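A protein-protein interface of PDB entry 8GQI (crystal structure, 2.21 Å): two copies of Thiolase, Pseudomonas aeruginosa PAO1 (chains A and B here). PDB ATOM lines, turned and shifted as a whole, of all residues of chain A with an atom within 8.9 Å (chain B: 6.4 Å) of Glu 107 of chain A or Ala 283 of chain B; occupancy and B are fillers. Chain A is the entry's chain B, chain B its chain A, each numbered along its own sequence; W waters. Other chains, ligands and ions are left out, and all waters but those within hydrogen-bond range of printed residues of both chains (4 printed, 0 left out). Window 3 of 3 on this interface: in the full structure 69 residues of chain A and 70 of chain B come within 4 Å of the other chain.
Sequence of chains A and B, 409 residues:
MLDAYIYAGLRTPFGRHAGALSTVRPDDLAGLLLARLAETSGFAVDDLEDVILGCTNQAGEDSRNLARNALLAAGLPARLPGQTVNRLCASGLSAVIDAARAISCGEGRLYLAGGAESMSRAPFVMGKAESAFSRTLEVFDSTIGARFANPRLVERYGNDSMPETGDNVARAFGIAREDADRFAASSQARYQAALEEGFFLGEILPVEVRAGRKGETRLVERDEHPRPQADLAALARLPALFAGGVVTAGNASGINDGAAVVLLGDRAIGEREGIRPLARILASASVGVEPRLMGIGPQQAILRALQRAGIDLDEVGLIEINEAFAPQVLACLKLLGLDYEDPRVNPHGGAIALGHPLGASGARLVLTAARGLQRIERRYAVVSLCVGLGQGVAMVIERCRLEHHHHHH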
ATOM      1  N   ASP A  47      29.741  12.526 -33.407  1.00  0.00           N
ATOM      2  CA  ASP A  47      29.390  12.901 -32.018  1.00  0.00           C
ATOM      3  C   ASP A  47      29.216  14.411 -31.871  1.00  0.00           C
ATOM      4  O   ASP A  47      28.863  14.859 -30.764  1.00  0.00           O
ATOM      5  CB  ASP A  47      30.476  12.443 -31.063  1.00  0.00           C
ATOM      6  CG  ASP A  47      30.633  10.933 -31.004  1.00  0.00           C
ATOM      7  OD1 ASP A  47      29.605  10.229 -31.147  1.00  0.00           O
ATOM      8  OD2 ASP A  47      31.793  10.486 -30.818  1.00  0.00           O
ATOM      9  N   LEU A  48      29.500  15.200 -32.907  1.00  0.00           N
ATOM     10  CA  LEU A  48      29.306  16.668 -32.784  1.00  0.00           C
ATOM     11  C   LEU A  48      27.823  16.914 -32.767  1.00  0.00           C
ATOM     12  O   LEU A  48      27.142  16.386 -33.621  1.00  0.00           O
ATOM     13  CB  LEU A  48      29.955  17.435 -33.927  1.00  0.00           C
ATOM     14  CG  LEU A  48      31.462  17.429 -33.907  1.00  0.00           C
ATOM     15  CD1 LEU A  48      31.973  17.849 -35.280  1.00  0.00           C
ATOM     16  CD2 LEU A  48      31.970  18.351 -32.798  1.00  0.00           C
ATOM     17  N   GLU A  49      27.372  17.680 -31.790  1.00  0.00           N
ATOM     18  CA  GLU A  49      25.942  17.970 -31.596  1.00  0.00           C
ATOM     19  C   GLU A  49      25.513  19.244 -32.334  1.00  0.00           C
ATOM     20  O   GLU A  49      24.389  19.279 -32.845  1.00  0.00           O
ATOM     21  CB  GLU A  49      25.664  18.119 -30.109  1.00  0.00           C
ATOM     22  CG  GLU A  49      24.188  18.207 -29.819  1.00  0.00           C
ATOM     23  CD  GLU A  49      23.456  16.878 -29.866  1.00  0.00           C
ATOM     24  OE1 GLU A  49      24.144  15.825 -30.004  1.00  0.00           O
ATOM     25  OE2 GLU A  49      22.200  16.903 -29.697  1.00  0.00           O
ATOM     26  N   ASP A  50      26.332  20.273 -32.347  1.00  0.00           N
ATOM     27  CA  ASP A  50      25.896  21.603 -32.845  1.00  0.00           C
ATOM     28  C   ASP A  50      27.135  22.454 -33.042  1.00  0.00           C
ATOM     29  O   ASP A  50      28.158  22.160 -32.411  1.00  0.00           O
ATOM     30  CB  ASP A  50      24.954  22.273 -31.828  1.00  0.00           C
ATOM     31  CG  ASP A  50      23.857  23.173 -32.392  1.00  0.00           C
ATOM     32  OD1 ASP A  50      23.949  23.604 -33.580  1.00  0.00           O
ATOM     33  OD2 ASP A  50      22.900  23.446 -31.629  1.00  0.00           O
ATOM     34  N   ILE A  52      28.161  26.500 -32.797  1.00  0.00           N
ATOM     35  CA  ILE A  52      27.635  27.803 -32.293  1.00  0.00           C
ATOM     36  C   ILE A  52      28.688  28.864 -32.589  1.00  0.00           C
ATOM     37  O   ILE A  52      29.760  28.801 -31.992  1.00  0.00           O
ATOM     38  CB  ILE A  52      27.260  27.753 -30.808  1.00  0.00           C
ATOM     39  CG1 ILE A  52      26.430  26.510 -30.506  1.00  0.00           C
ATOM     40  CG2 ILE A  52      26.513  29.009 -30.361  1.00  0.00           C
ATOM     41  CD1 ILE A  52      25.942  26.417 -29.095  1.00  0.00           C
ATOM     42  N   ASP A  98      27.326  29.280 -24.236  1.00  0.00           N
ATOM     43  CA  ASP A  98      26.047  28.612 -24.594  1.00  0.00           C
ATOM     44  C   ASP A  98      26.318  27.122 -24.856  1.00  0.00           C
ATOM     45  O   ASP A  98      25.523  26.314 -24.382  1.00  0.00           O
ATOM     46  CB  ASP A  98      25.354  29.249 -25.805  1.00  0.00           C
ATOM     47  CG  ASP A  98      24.588  30.546 -25.534  1.00  0.00           C
ATOM     48  OD1 ASP A  98      24.063  30.708 -24.379  1.00  0.00           O
ATOM     49  OD2 ASP A  98      24.473  31.393 -26.501  1.00  0.00           O
ATOM     50  N   ALA A  99      27.345  26.778 -25.634  1.00  0.00           N
ATOM     51  CA  ALA A  99      27.796  25.388 -25.830  1.00  0.00           C
ATOM     52  C   ALA A  99      28.160  24.765 -24.458  1.00  0.00           C
ATOM     53  O   ALA A  99      27.745  23.658 -24.209  1.00  0.00           O
ATOM     54  CB  ALA A  99      28.946  25.349 -26.787  1.00  0.00           C
ATOM     55  N   ALA A 100      28.814  25.484 -23.551  1.00  0.00           N
ATOM     56  CA  ALA A 100      29.221  24.925 -22.241  1.00  0.00           C
ATOM     57  C   ALA A 100      27.974  24.563 -21.423  1.00  0.00           C
ATOM     58  O   ALA A 100      27.943  23.473 -20.827  1.00  0.00           O
ATOM     59  CB  ALA A 100      30.136  25.864 -21.503  1.00  0.00           C
ATOM     60  N   ARG A 101      26.970  25.432 -21.426  1.00  0.00           N
ATOM     61  CA  ARG A 101      25.683  25.236 -20.718  1.00  0.00           C
ATOM     62  C   ARG A 101      24.940  24.051 -21.320  1.00  0.00           C
ATOM     63  O   ARG A 101      24.397  23.212 -20.530  1.00  0.00           O
ATOM     64  CB  ARG A 101      24.822  26.489 -20.780  1.00  0.00           C
ATOM     65  CG  ARG A 101      25.376  27.623 -19.941  1.00  0.00           C
ATOM     66  CD  ARG A 101      24.767  28.934 -20.402  1.00  0.00           C
ATOM     67  NE  ARG A 101      25.007  29.967 -19.422  1.00  0.00           N
ATOM     68  CZ  ARG A 101      24.578  31.211 -19.511  1.00  0.00           C
ATOM     69  NH1 ARG A 101      23.887  31.596 -20.564  1.00  0.00           N
ATOM     70  NH2 ARG A 101      24.844  32.066 -18.538  1.00  0.00           N
ATOM     71  N   ALA A 102      24.863  24.007 -22.645  1.00  0.00           N
ATOM     72  CA  ALA A 102      24.251  22.863 -23.349  1.00  0.00           C
ATOM     73  C   ALA A 102      24.874  21.562 -22.824  1.00  0.00           C
ATOM     74  O   ALA A 102      24.122  20.665 -22.489  1.00  0.00           O
ATOM     75  CB  ALA A 102      24.420  22.973 -24.838  1.00  0.00           C
ATOM     76  N   ILE A 103      26.206  21.464 -22.850  1.00  0.00           N
ATOM     77  CA  ILE A 103      26.956  20.257 -22.419  1.00  0.00           C
ATOM     78  C   ILE A 103      26.623  19.958 -20.946  1.00  0.00           C
ATOM     79  O   ILE A 103      26.385  18.755 -20.621  1.00  0.00           O
ATOM     80  CB  ILE A 103      28.470  20.435 -22.651  1.00  0.00           C
ATOM     81  CG1 ILE A 103      28.845  20.417 -24.136  1.00  0.00           C
ATOM     82  CG2 ILE A 103      29.251  19.374 -21.895  1.00  0.00           C
ATOM     83  CD1 ILE A 103      30.128  21.116 -24.406  1.00  0.00           C
ATOM     84  N   SER A 104      26.625  20.995 -20.093  1.00  0.00           N
ATOM     85  CA  SER A 104      26.435  20.903 -18.626  1.00  0.00           C
ATOM     86  C   SER A 104      25.050  20.310 -18.312  1.00  0.00           C
ATOM     87  O   SER A 104      24.886  19.697 -17.273  1.00  0.00           O
ATOM     88  CB  SER A 104      26.644  22.255 -17.985  1.00  0.00           C
ATOM     89  OG  SER A 104      27.994  22.660 -18.154  1.00  0.00           O
ATOM     90  N   CYS A 105      24.093  20.532 -19.205  1.00  0.00           N
ATOM     91  CA  CYS A 105      22.701  20.030 -19.137  1.00  0.00           C
ATOM     92  C   CYS A 105      22.565  18.627 -19.664  1.00  0.00           C
ATOM     93  O   CYS A 105      21.458  18.162 -19.594  1.00  0.00           O
ATOM     94  CB  CYS A 105      21.777  20.804 -20.066  1.00  0.00           C
ATOM     95  SG  CYS A 105      21.429  22.356 -19.276  1.00  0.00           S
ATOM     96  N   GLY A 106      23.591  18.062 -20.276  1.00  0.00           N
ATOM     97  CA  GLY A 106      23.469  16.739 -20.906  1.00  0.00           C
ATOM     98  C   GLY A 106      22.846  16.805 -22.276  1.00  0.00           C
ATOM     99  O   GLY A 106      22.396  15.737 -22.728  1.00  0.00           O
ATOM    100  N   GLU A 107      22.853  17.975 -22.960  1.00  0.00           N
ATOM    101  CA  GLU A 107      22.258  18.074 -24.321  1.00  0.00           C
ATOM    102  C   GLU A 107      23.405  18.109 -25.320  1.00  0.00           C
ATOM    103  O   GLU A 107      23.787  19.204 -25.708  1.00  0.00           O
ATOM    104  CB  GLU A 107      21.259  19.237 -24.455  1.00  0.00           C
ATOM    105  CG  GLU A 107      19.975  18.960 -23.668  1.00  0.00           C
ATOM    106  CD  GLU A 107      18.667  19.634 -24.038  1.00  0.00           C
ATOM    107  OE1 GLU A 107      18.686  20.789 -24.634  1.00  0.00           O
ATOM    108  OE2 GLU A 107      17.602  19.001 -23.700  1.00  0.00           O
ATOM    109  N   GLY A 108      23.946  16.922 -25.628  1.00  0.00           N
ATOM    110  CA  GLY A 108      25.076  16.684 -26.539  1.00  0.00           C
ATOM    111  C   GLY A 108      26.381  16.591 -25.776  1.00  0.00           C
ATOM    112  O   GLY A 108      26.496  17.201 -24.674  1.00  0.00           O
ATOM    113  N   ARG A 109      27.335  15.867 -26.346  1.00  0.00           N
ATOM    114  CA  ARG A 109      28.611  15.504 -25.687  1.00  0.00           C
ATOM    115  C   ARG A 109      29.756  16.365 -26.236  1.00  0.00           C
ATOM    116  O   ARG A 109      30.824  16.413 -25.595  1.00  0.00           O
ATOM    117  CB  ARG A 109      28.877  14.021 -25.939  1.00  0.00           C
ATOM    118  CG  ARG A 109      28.038  13.112 -25.050  1.00  0.00           C
ATOM    119  CD  ARG A 109      28.111  11.625 -25.392  1.00  0.00           C
ATOM    120  NE  ARG A 109      27.249  10.762 -24.566  1.00  0.00           N
ATOM    121  CZ  ARG A 109      27.439  10.495 -23.257  1.00  0.00           C
ATOM    122  NH1 ARG A 109      28.450  11.033 -22.582  1.00  0.00           N
ATOM    123  NH2 ARG A 109      26.613   9.683 -22.619  1.00  0.00           N
ATOM    124  N   LEU A 110      29.539  16.991 -27.393  1.00  0.00           N
ATOM    125  CA  LEU A 110      30.614  17.611 -28.202  1.00  0.00           C
ATOM    126  C   LEU A 110      30.032  18.792 -28.994  1.00  0.00           C
ATOM    127  O   LEU A 110      29.074  18.590 -29.755  1.00  0.00           O
ATOM    128  CB  LEU A 110      31.150  16.496 -29.119  1.00  0.00           C
ATOM    129  CG  LEU A 110      32.607  16.563 -29.542  1.00  0.00           C
ATOM    130  CD1 LEU A 110      33.550  16.816 -28.374  1.00  0.00           C
ATOM    131  CD2 LEU A 110      32.985  15.290 -30.277  1.00  0.00           C
ATOM    132  N   TYR A 111      30.612  19.973 -28.849  1.00  0.00           N
ATOM    133  CA  TYR A 111      30.197  21.198 -29.588  1.00  0.00           C
ATOM    134  C   TYR A 111      31.427  21.890 -30.199  1.00  0.00           C
ATOM    135  O   TYR A 111      32.483  21.948 -29.589  1.00  0.00           O
ATOM    136  CB  TYR A 111      29.506  22.196 -28.647  1.00  0.00           C
ATOM    137  CG  TYR A 111      28.098  21.854 -28.259  1.00  0.00           C
ATOM    138  CD1 TYR A 111      27.801  20.752 -27.466  1.00  0.00           C
ATOM    139  CD2 TYR A 111      27.052  22.633 -28.699  1.00  0.00           C
ATOM    140  CE1 TYR A 111      26.490  20.429 -27.146  1.00  0.00           C
ATOM    141  CE2 TYR A 111      25.742  22.342 -28.382  1.00  0.00           C
ATOM    142  CZ  TYR A 111      25.461  21.218 -27.613  1.00  0.00           C
ATOM    143  OH  TYR A 111      24.159  20.966 -27.327  1.00  0.00           O
ATOM    144  N   ASP A 266      31.839  16.950 -22.894  1.00  0.00           N
ATOM    145  CA  ASP A 266      31.751  16.418 -21.500  1.00  0.00           C
ATOM    146  C   ASP A 266      33.059  15.698 -21.162  1.00  0.00           C
ATOM    147  O   ASP A 266      33.918  15.530 -22.070  1.00  0.00           O
ATOM    148  CB  ASP A 266      30.510  15.549 -21.289  1.00  0.00           C
ATOM    149  CG  ASP A 266      30.460  14.237 -22.070  1.00  0.00           C
ATOM    150  OD1 ASP A 266      31.447  13.875 -22.705  1.00  0.00           O
ATOM    151  OD2 ASP A 266      29.426  13.579 -22.031  1.00  0.00           O
ATOM    152  N   MET B   1      17.389  15.980 -17.694  1.00  0.00           N
ATOM    153  CA  MET B   1      16.114  16.711 -17.846  1.00  0.00           C
ATOM    154  C   MET B   1      16.378  18.202 -17.640  1.00  0.00           C
ATOM    155  O   MET B   1      16.995  18.523 -16.622  1.00  0.00           O
ATOM    156  CB  MET B   1      15.089  16.256 -16.805  1.00  0.00           C
ATOM    157  CG  MET B   1      13.675  16.367 -17.288  1.00  0.00           C
ATOM    158  SD  MET B   1      13.434  15.270 -18.707  1.00  0.00           S
ATOM    159  CE  MET B   1      13.517  13.669 -17.893  1.00  0.00           C
ATOM    160  N   LEU B   2      15.922  19.079 -18.544  1.00  0.00           N
ATOM    161  CA  LEU B   2      16.018  20.534 -18.288  1.00  0.00           C
ATOM    162  C   LEU B   2      15.154  20.821 -17.061  1.00  0.00           C
ATOM    163  O   LEU B   2      14.291  20.045 -16.776  1.00  0.00           O
ATOM    164  CB  LEU B   2      15.571  21.323 -19.516  1.00  0.00           C
ATOM    165  CG  LEU B   2      16.364  21.074 -20.793  1.00  0.00           C
ATOM    166  CD1 LEU B   2      15.895  21.970 -21.915  1.00  0.00           C
ATOM    167  CD2 LEU B   2      17.856  21.273 -20.568  1.00  0.00           C
ATOM    168  N   ILE B  97      15.120  27.742 -25.595  1.00  0.00           N
ATOM    169  CA  ILE B  97      16.051  26.637 -25.314  1.00  0.00           C
ATOM    170  C   ILE B  97      17.329  27.158 -24.643  1.00  0.00           C
ATOM    171  O   ILE B  97      17.745  26.566 -23.620  1.00  0.00           O
ATOM    172  CB  ILE B  97      16.330  25.834 -26.587  1.00  0.00           C
ATOM    173  CG1 ILE B  97      15.073  25.061 -27.003  1.00  0.00           C
ATOM    174  CG2 ILE B  97      17.516  24.920 -26.342  1.00  0.00           C
ATOM    175  CD1 ILE B  97      15.180  24.354 -28.375  1.00  0.00           C
ATOM    176  N   ARG B 101      18.402  26.204 -20.746  1.00  0.00           N
ATOM    177  CA  ARG B 101      19.723  25.618 -20.444  1.00  0.00           C
ATOM    178  C   ARG B 101      20.471  26.481 -19.418  1.00  0.00           C
ATOM    179  O   ARG B 101      21.084  25.887 -18.470  1.00  0.00           O
ATOM    180  CB  ARG B 101      20.553  25.378 -21.704  1.00  0.00           C
ATOM    181  CG  ARG B 101      20.026  24.244 -22.572  1.00  0.00           C
ATOM    182  CD  ARG B 101      20.626  24.340 -23.949  1.00  0.00           C
ATOM    183  NE  ARG B 101      20.248  23.206 -24.750  1.00  0.00           N
ATOM    184  CZ  ARG B 101      20.689  22.958 -25.963  1.00  0.00           C
ATOM    185  NH1 ARG B 101      21.505  23.809 -26.573  1.00  0.00           N
ATOM    186  NH2 ARG B 101      20.320  21.850 -26.562  1.00  0.00           N
ATOM    187  N   ILE B 281       9.852  23.157 -18.954  1.00  0.00           N
ATOM    188  CA  ILE B 281      10.672  22.683 -20.105  1.00  0.00           C
ATOM    189  C   ILE B 281      11.456  21.432 -19.672  1.00  0.00           C
ATOM    190  O   ILE B 281      12.225  21.520 -18.735  1.00  0.00           O
ATOM    191  CB  ILE B 281      11.573  23.825 -20.631  1.00  0.00           C
ATOM    192  CG1 ILE B 281      10.703  25.054 -20.916  1.00  0.00           C
ATOM    193  CG2 ILE B 281      12.362  23.329 -21.844  1.00  0.00           C
ATOM    194  CD1 ILE B 281      11.426  26.202 -21.586  1.00  0.00           C
ATOM    195  N   LEU B 282      11.274  20.331 -20.387  1.00  0.00           N
ATOM    196  CA  LEU B 282      11.868  19.010 -20.083  1.00  0.00           C
ATOM    197  C   LEU B 282      13.115  18.769 -20.917  1.00  0.00           C
ATOM    198  O   LEU B 282      14.117  18.241 -20.338  1.00  0.00           O
ATOM    199  CB  LEU B 282      10.847  17.924 -20.420  1.00  0.00           C
ATOM    200  CG  LEU B 282       9.657  17.891 -19.472  1.00  0.00           C
ATOM    201  CD1 LEU B 282       8.807  16.658 -19.733  1.00  0.00           C
ATOM    202  CD2 LEU B 282      10.151  17.948 -18.025  1.00  0.00           C
ATOM    203  N   ALA B 283      13.053  19.107 -22.210  1.00  0.00           N
ATOM    204  CA  ALA B 283      14.092  18.701 -23.171  1.00  0.00           C
ATOM    205  C   ALA B 283      13.939  19.433 -24.499  1.00  0.00           C
ATOM    206  O   ALA B 283      12.842  19.801 -24.876  1.00  0.00           O
ATOM    207  CB  ALA B 283      14.018  17.211 -23.377  1.00  0.00           C
ATOM    208  N   SER B 284      15.048  19.533 -25.218  1.00  0.00           N
ATOM    209  CA  SER B 284      15.086  20.013 -26.617  1.00  0.00           C
ATOM    210  C   SER B 284      16.005  19.101 -27.411  1.00  0.00           C
ATOM    211  O   SER B 284      16.757  18.336 -26.805  1.00  0.00           O
ATOM    212  CB  SER B 284      15.540  21.419 -26.649  1.00  0.00           C
ATOM    213  OG  SER B 284      16.952  21.439 -26.591  1.00  0.00           O
ATOM    214  N   ALA B 285      15.904  19.161 -28.727  1.00  0.00           N
ATOM    215  CA  ALA B 285      16.833  18.516 -29.661  1.00  0.00           C
ATOM    216  C   ALA B 285      16.916  19.380 -30.910  1.00  0.00           C
ATOM    217  O   ALA B 285      15.896  19.960 -31.279  1.00  0.00           O
ATOM    218  CB  ALA B 285      16.389  17.136 -30.004  1.00  0.00           C
ATOM    219  N   ARG B 304      13.969  12.792 -30.956  1.00  0.00           N
ATOM    220  CA  ARG B 304      15.100  12.972 -30.015  1.00  0.00           C
ATOM    221  C   ARG B 304      14.647  13.742 -28.771  1.00  0.00           C
ATOM    222  O   ARG B 304      15.104  13.371 -27.651  1.00  0.00           O
ATOM    223  CB  ARG B 304      16.265  13.714 -30.680  1.00  0.00           C
ATOM    224  CG  ARG B 304      16.942  12.931 -31.798  1.00  0.00           C
ATOM    225  CD  ARG B 304      18.147  13.689 -32.336  1.00  0.00           C
ATOM    226  NE  ARG B 304      19.259  13.561 -31.410  1.00  0.00           N
ATOM    227  CZ  ARG B 304      20.199  14.481 -31.166  1.00  0.00           C
ATOM    228  NH1 ARG B 304      20.191  15.663 -31.758  1.00  0.00           N
ATOM    229  NH2 ARG B 304      21.139  14.206 -30.276  1.00  0.00           N
ATOM    230  N   ALA B 305      13.849  14.807 -28.931  1.00  0.00           N
ATOM    231  CA  ALA B 305      13.329  15.557 -27.778  1.00  0.00           C
ATOM    232  C   ALA B 305      12.472  14.631 -26.872  1.00  0.00           C
ATOM    233  O   ALA B 305      12.537  14.775 -25.620  1.00  0.00           O
ATOM    234  CB  ALA B 305      12.569  16.777 -28.259  1.00  0.00           C
ATOM    235  N   LEU B 306      11.600  13.796 -27.462  1.00  0.00           N
ATOM    236  CA  LEU B 306      10.683  12.908 -26.696  1.00  0.00           C
ATOM    237  C   LEU B 306      11.579  11.912 -25.946  1.00  0.00           C
ATOM    238  O   LEU B 306      11.379  11.739 -24.746  1.00  0.00           O
ATOM    239  CB  LEU B 306       9.703  12.163 -27.609  1.00  0.00           C
ATOM    240  CG  LEU B 306       8.627  13.010 -28.288  1.00  0.00           C
ATOM    241  CD1 LEU B 306       7.872  12.172 -29.301  1.00  0.00           C
ATOM    242  CD2 LEU B 306       7.698  13.683 -27.300  1.00  0.00           C
ATOM    243  N   GLN B 307      12.590  11.375 -26.622  1.00  0.00           N
ATOM    244  CA  GLN B 307      13.521  10.399 -26.015  1.00  0.00           C
ATOM    245  C   GLN B 307      14.243  11.081 -24.839  1.00  0.00           C
ATOM    246  O   GLN B 307      14.316  10.480 -23.748  1.00  0.00           O
ATOM    247  CB  GLN B 307      14.404   9.821 -27.118  1.00  0.00           C
ATOM    248  CG  GLN B 307      15.248   8.624 -26.693  1.00  0.00           C
ATOM    249  CD  GLN B 307      16.437   8.999 -25.834  1.00  0.00           C
ATOM    250  OE1 GLN B 307      16.824   8.268 -24.919  1.00  0.00           O
ATOM    251  NE2 GLN B 307      17.026  10.156 -26.112  1.00  0.00           N
ATOM    252  N   ARG B 308      14.716  12.311 -24.995  1.00  0.00           N
ATOM    253  CA  ARG B 308      15.436  12.988 -23.893  1.00  0.00           C
ATOM    254  C   ARG B 308      14.461  13.276 -22.766  1.00  0.00           C
ATOM    255  O   ARG B 308      14.934  13.332 -21.635  1.00  0.00           O
ATOM    256  CB  ARG B 308      16.085  14.311 -24.292  1.00  0.00           C
ATOM    257  CG  ARG B 308      17.284  14.118 -25.184  1.00  0.00           C
ATOM    258  CD  ARG B 308      17.811  15.427 -25.703  1.00  0.00           C
ATOM    259  NE  ARG B 308      19.124  15.213 -26.274  1.00  0.00           N
ATOM    260  CZ  ARG B 308      19.812  16.079 -27.028  1.00  0.00           C
ATOM    261  NH1 ARG B 308      19.294  17.242 -27.394  1.00  0.00           N
ATOM    262  NH2 ARG B 308      21.033  15.749 -27.424  1.00  0.00           N
ATOM    263  N   ALA B 309      13.187  13.510 -23.086  1.00  0.00           N
ATOM    264  CA  ALA B 309      12.166  13.879 -22.093  1.00  0.00           C
ATOM    265  C   ALA B 309      11.655  12.613 -21.387  1.00  0.00           C
ATOM    266  O   ALA B 309      10.991  12.783 -20.384  1.00  0.00           O
ATOM    267  CB  ALA B 309      11.042  14.645 -22.744  1.00  0.00           C
ATOM    268  N   GLY B 310      11.933  11.416 -21.923  1.00  0.00           N
ATOM    269  CA  GLY B 310      11.477  10.119 -21.390  1.00  0.00           C
ATOM    270  C   GLY B 310       9.993   9.890 -21.580  1.00  0.00           C
ATOM    271  O   GLY B 310       9.401   9.160 -20.768  1.00  0.00           O
ATOM    272  N   ALA B 394      13.139  20.884 -31.803  1.00  0.00           N
ATOM    273  CA  ALA B 394      11.937  20.449 -31.057  1.00  0.00           C
ATOM    274  C   ALA B 394      12.141  20.687 -29.572  1.00  0.00           C
ATOM    275  O   ALA B 394      13.272  20.655 -29.104  1.00  0.00           O
ATOM    276  CB  ALA B 394      11.623  19.020 -31.375  1.00  0.00           C
ATOM    277  N   MET B 395      11.060  20.933 -28.842  1.00  0.00           N
ATOM    278  CA  MET B 395      11.126  21.104 -27.389  1.00  0.00           C
ATOM    279  C   MET B 395       9.911  20.405 -26.802  1.00  0.00           C
ATOM    280  O   MET B 395       8.841  20.553 -27.365  1.00  0.00           O
ATOM    281  CB  MET B 395      11.157  22.577 -26.998  1.00  0.00           C
ATOM    282  CG  MET B 395      11.461  22.781 -25.535  1.00  0.00           C
ATOM    283  SD  MET B 395      11.547  24.530 -25.089  1.00  0.00           S
ATOM    284  CE  MET B 395       9.812  24.906 -25.134  1.00  0.00           C
ATOM    285  N   VAL B 396      10.099  19.645 -25.721  1.00  0.00           N
ATOM    286  CA  VAL B 396       8.983  19.036 -24.928  1.00  0.00           C
ATOM    287  C   VAL B 396       8.689  19.878 -23.681  1.00  0.00           C
ATOM    288  O   VAL B 396       9.625  20.154 -22.957  1.00  0.00           O
ATOM    289  CB  VAL B 396       9.342  17.612 -24.515  1.00  0.00           C
ATOM    290  CG1 VAL B 396       8.195  16.967 -23.767  1.00  0.00           C
ATOM    291  CG2 VAL B 396       9.696  16.799 -25.745  1.00  0.00           C
ATOM    292  N   ILE B 397       7.425  20.191 -23.399  1.00  0.00           N
ATOM    293  CA  ILE B 397       7.052  20.844 -22.109  1.00  0.00           C
ATOM    294  C   ILE B 397       5.960  20.041 -21.420  1.00  0.00           C
ATOM    295  O   ILE B 397       5.284  19.201 -22.069  1.00  0.00           O
ATOM    296  CB  ILE B 397       6.619  22.304 -22.311  1.00  0.00           C
ATOM    297  CG1 ILE B 397       5.260  22.367 -22.990  1.00  0.00           C
ATOM    298  CG2 ILE B 397       7.688  23.068 -23.094  1.00  0.00           C
ATOM    299  CD1 ILE B 397       4.747  23.772 -23.117  1.00  0.00           C
HETATM  300  O   HOH W   1      20.317  19.062 -29.416  1.00  0.00           O
HETATM  301  O   HOH W   2      22.383  17.545 -33.191  1.00  0.00           O
HETATM  302  O   HOH W   3      22.048  21.587 -29.398  1.00  0.00           O
HETATM  303  O   HOH W   4      22.723  24.647 -29.298  1.00  0.00           O
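Glu 107 of chain A touches just these residues of chain B: Leu 2, Arg 101, Ala 283, Ser 284 and Arg 308. Of the printed residues of chain B, Gly 108 of chain A touches Arg 308. Met 1 of chain B touches none of the printed residues of chain A. Of the printed residues of chain A, Ala 283 of chain B touches Glu 107. Of chain A, only Glu 107 comes within 4 Å of Ser 284 of chain B. Of the printed residues of chain A, Arg 304 of chain B touches Glu 49. The nearest residue of chain B that does not touch Glu 107 of chain A is Ile 97 of chain B (4.6 Å). The nearest printed residue of chain B that does not touch Ala 102 of chain A is Leu 2 of chain B (6.6 Å).
The guanidinium group of Arg 101 of chain B lies within hydrogen-bond range of the side-chain hydroxyl of Ser 284 of chain B. O of Leu 110 of chain A is in hydrogen-bond range of N of Glu 49 of chain A (2.8 Å). The backbone carbonyl oxygen of Glu 107 of chain A lies within hydrogen-bond range of the side-chain hydroxyl of Tyr 111 of chain A (2.4 Å).
Position printed for both chains: 101.
CB of Ala 102 of chain A touches NH1 of Arg 101 of chain B, at 3.5 Å. Cys 105 of chain A touches Leu 2 of chain B. CG of Leu 2 of chain B touches OE2 of Glu 107 of chain A, 3.8 Å away. Glu 107 of chain A touches Ala 283 of chain B. Arg 308 of chain B touches Glu 107 of chain A. Gly 108 of chain A touches Arg 308 of chain B. Tyr 111 of chain A touches Arg 101 of chain B.
SG of Cys 105 of chain A lies within hydrogen-bond range of O of Arg 101 of chain B, at 3.6 Å. The side-chain carboxylate of Glu 107 of chain A lies within salt-bridge range of the guanidinium group of Arg 101 of chain B (2.7 Å). OG of Ser 284 of chain B lies within hydrogen-bond range of OE1 of Glu 107 of chain A, at 2.7 Å. NH2 of Arg 304 of chain B lies within salt-bridge range of OE2 of Glu 49 of chain A, at 3.0 Å. The guanidinium group (NH2) of Arg 308 of chain B lies within salt-bridge range of the side-chain carboxylate (OE2) of Glu 49 of chain A (2.8 Å).
Water W2 lies within hydrogen-bond range of the backbone carbonyl oxygen of Glu 49 of chain A (2.7 Å) and the guanidinium group of Arg 304 of chain B (3.2 Å).
Printed residues of chain B that touch a printed residue of chain A: Leu 2, Arg 101, Ala 283, Ser 284, Arg 304 and Arg 308. Among the printed residues, 12 pairs touch across the chains. Among the printed residues, Asp or Glu carboxylates within 4 Å of a Lys or Arg side-chain nitrogen of the other chain: Glu 49 of chain A with Arg 304 of chain B, Glu 49 of chain A with Arg 308 of chain B and Glu 107 of chain A with Arg 101 of chain B.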
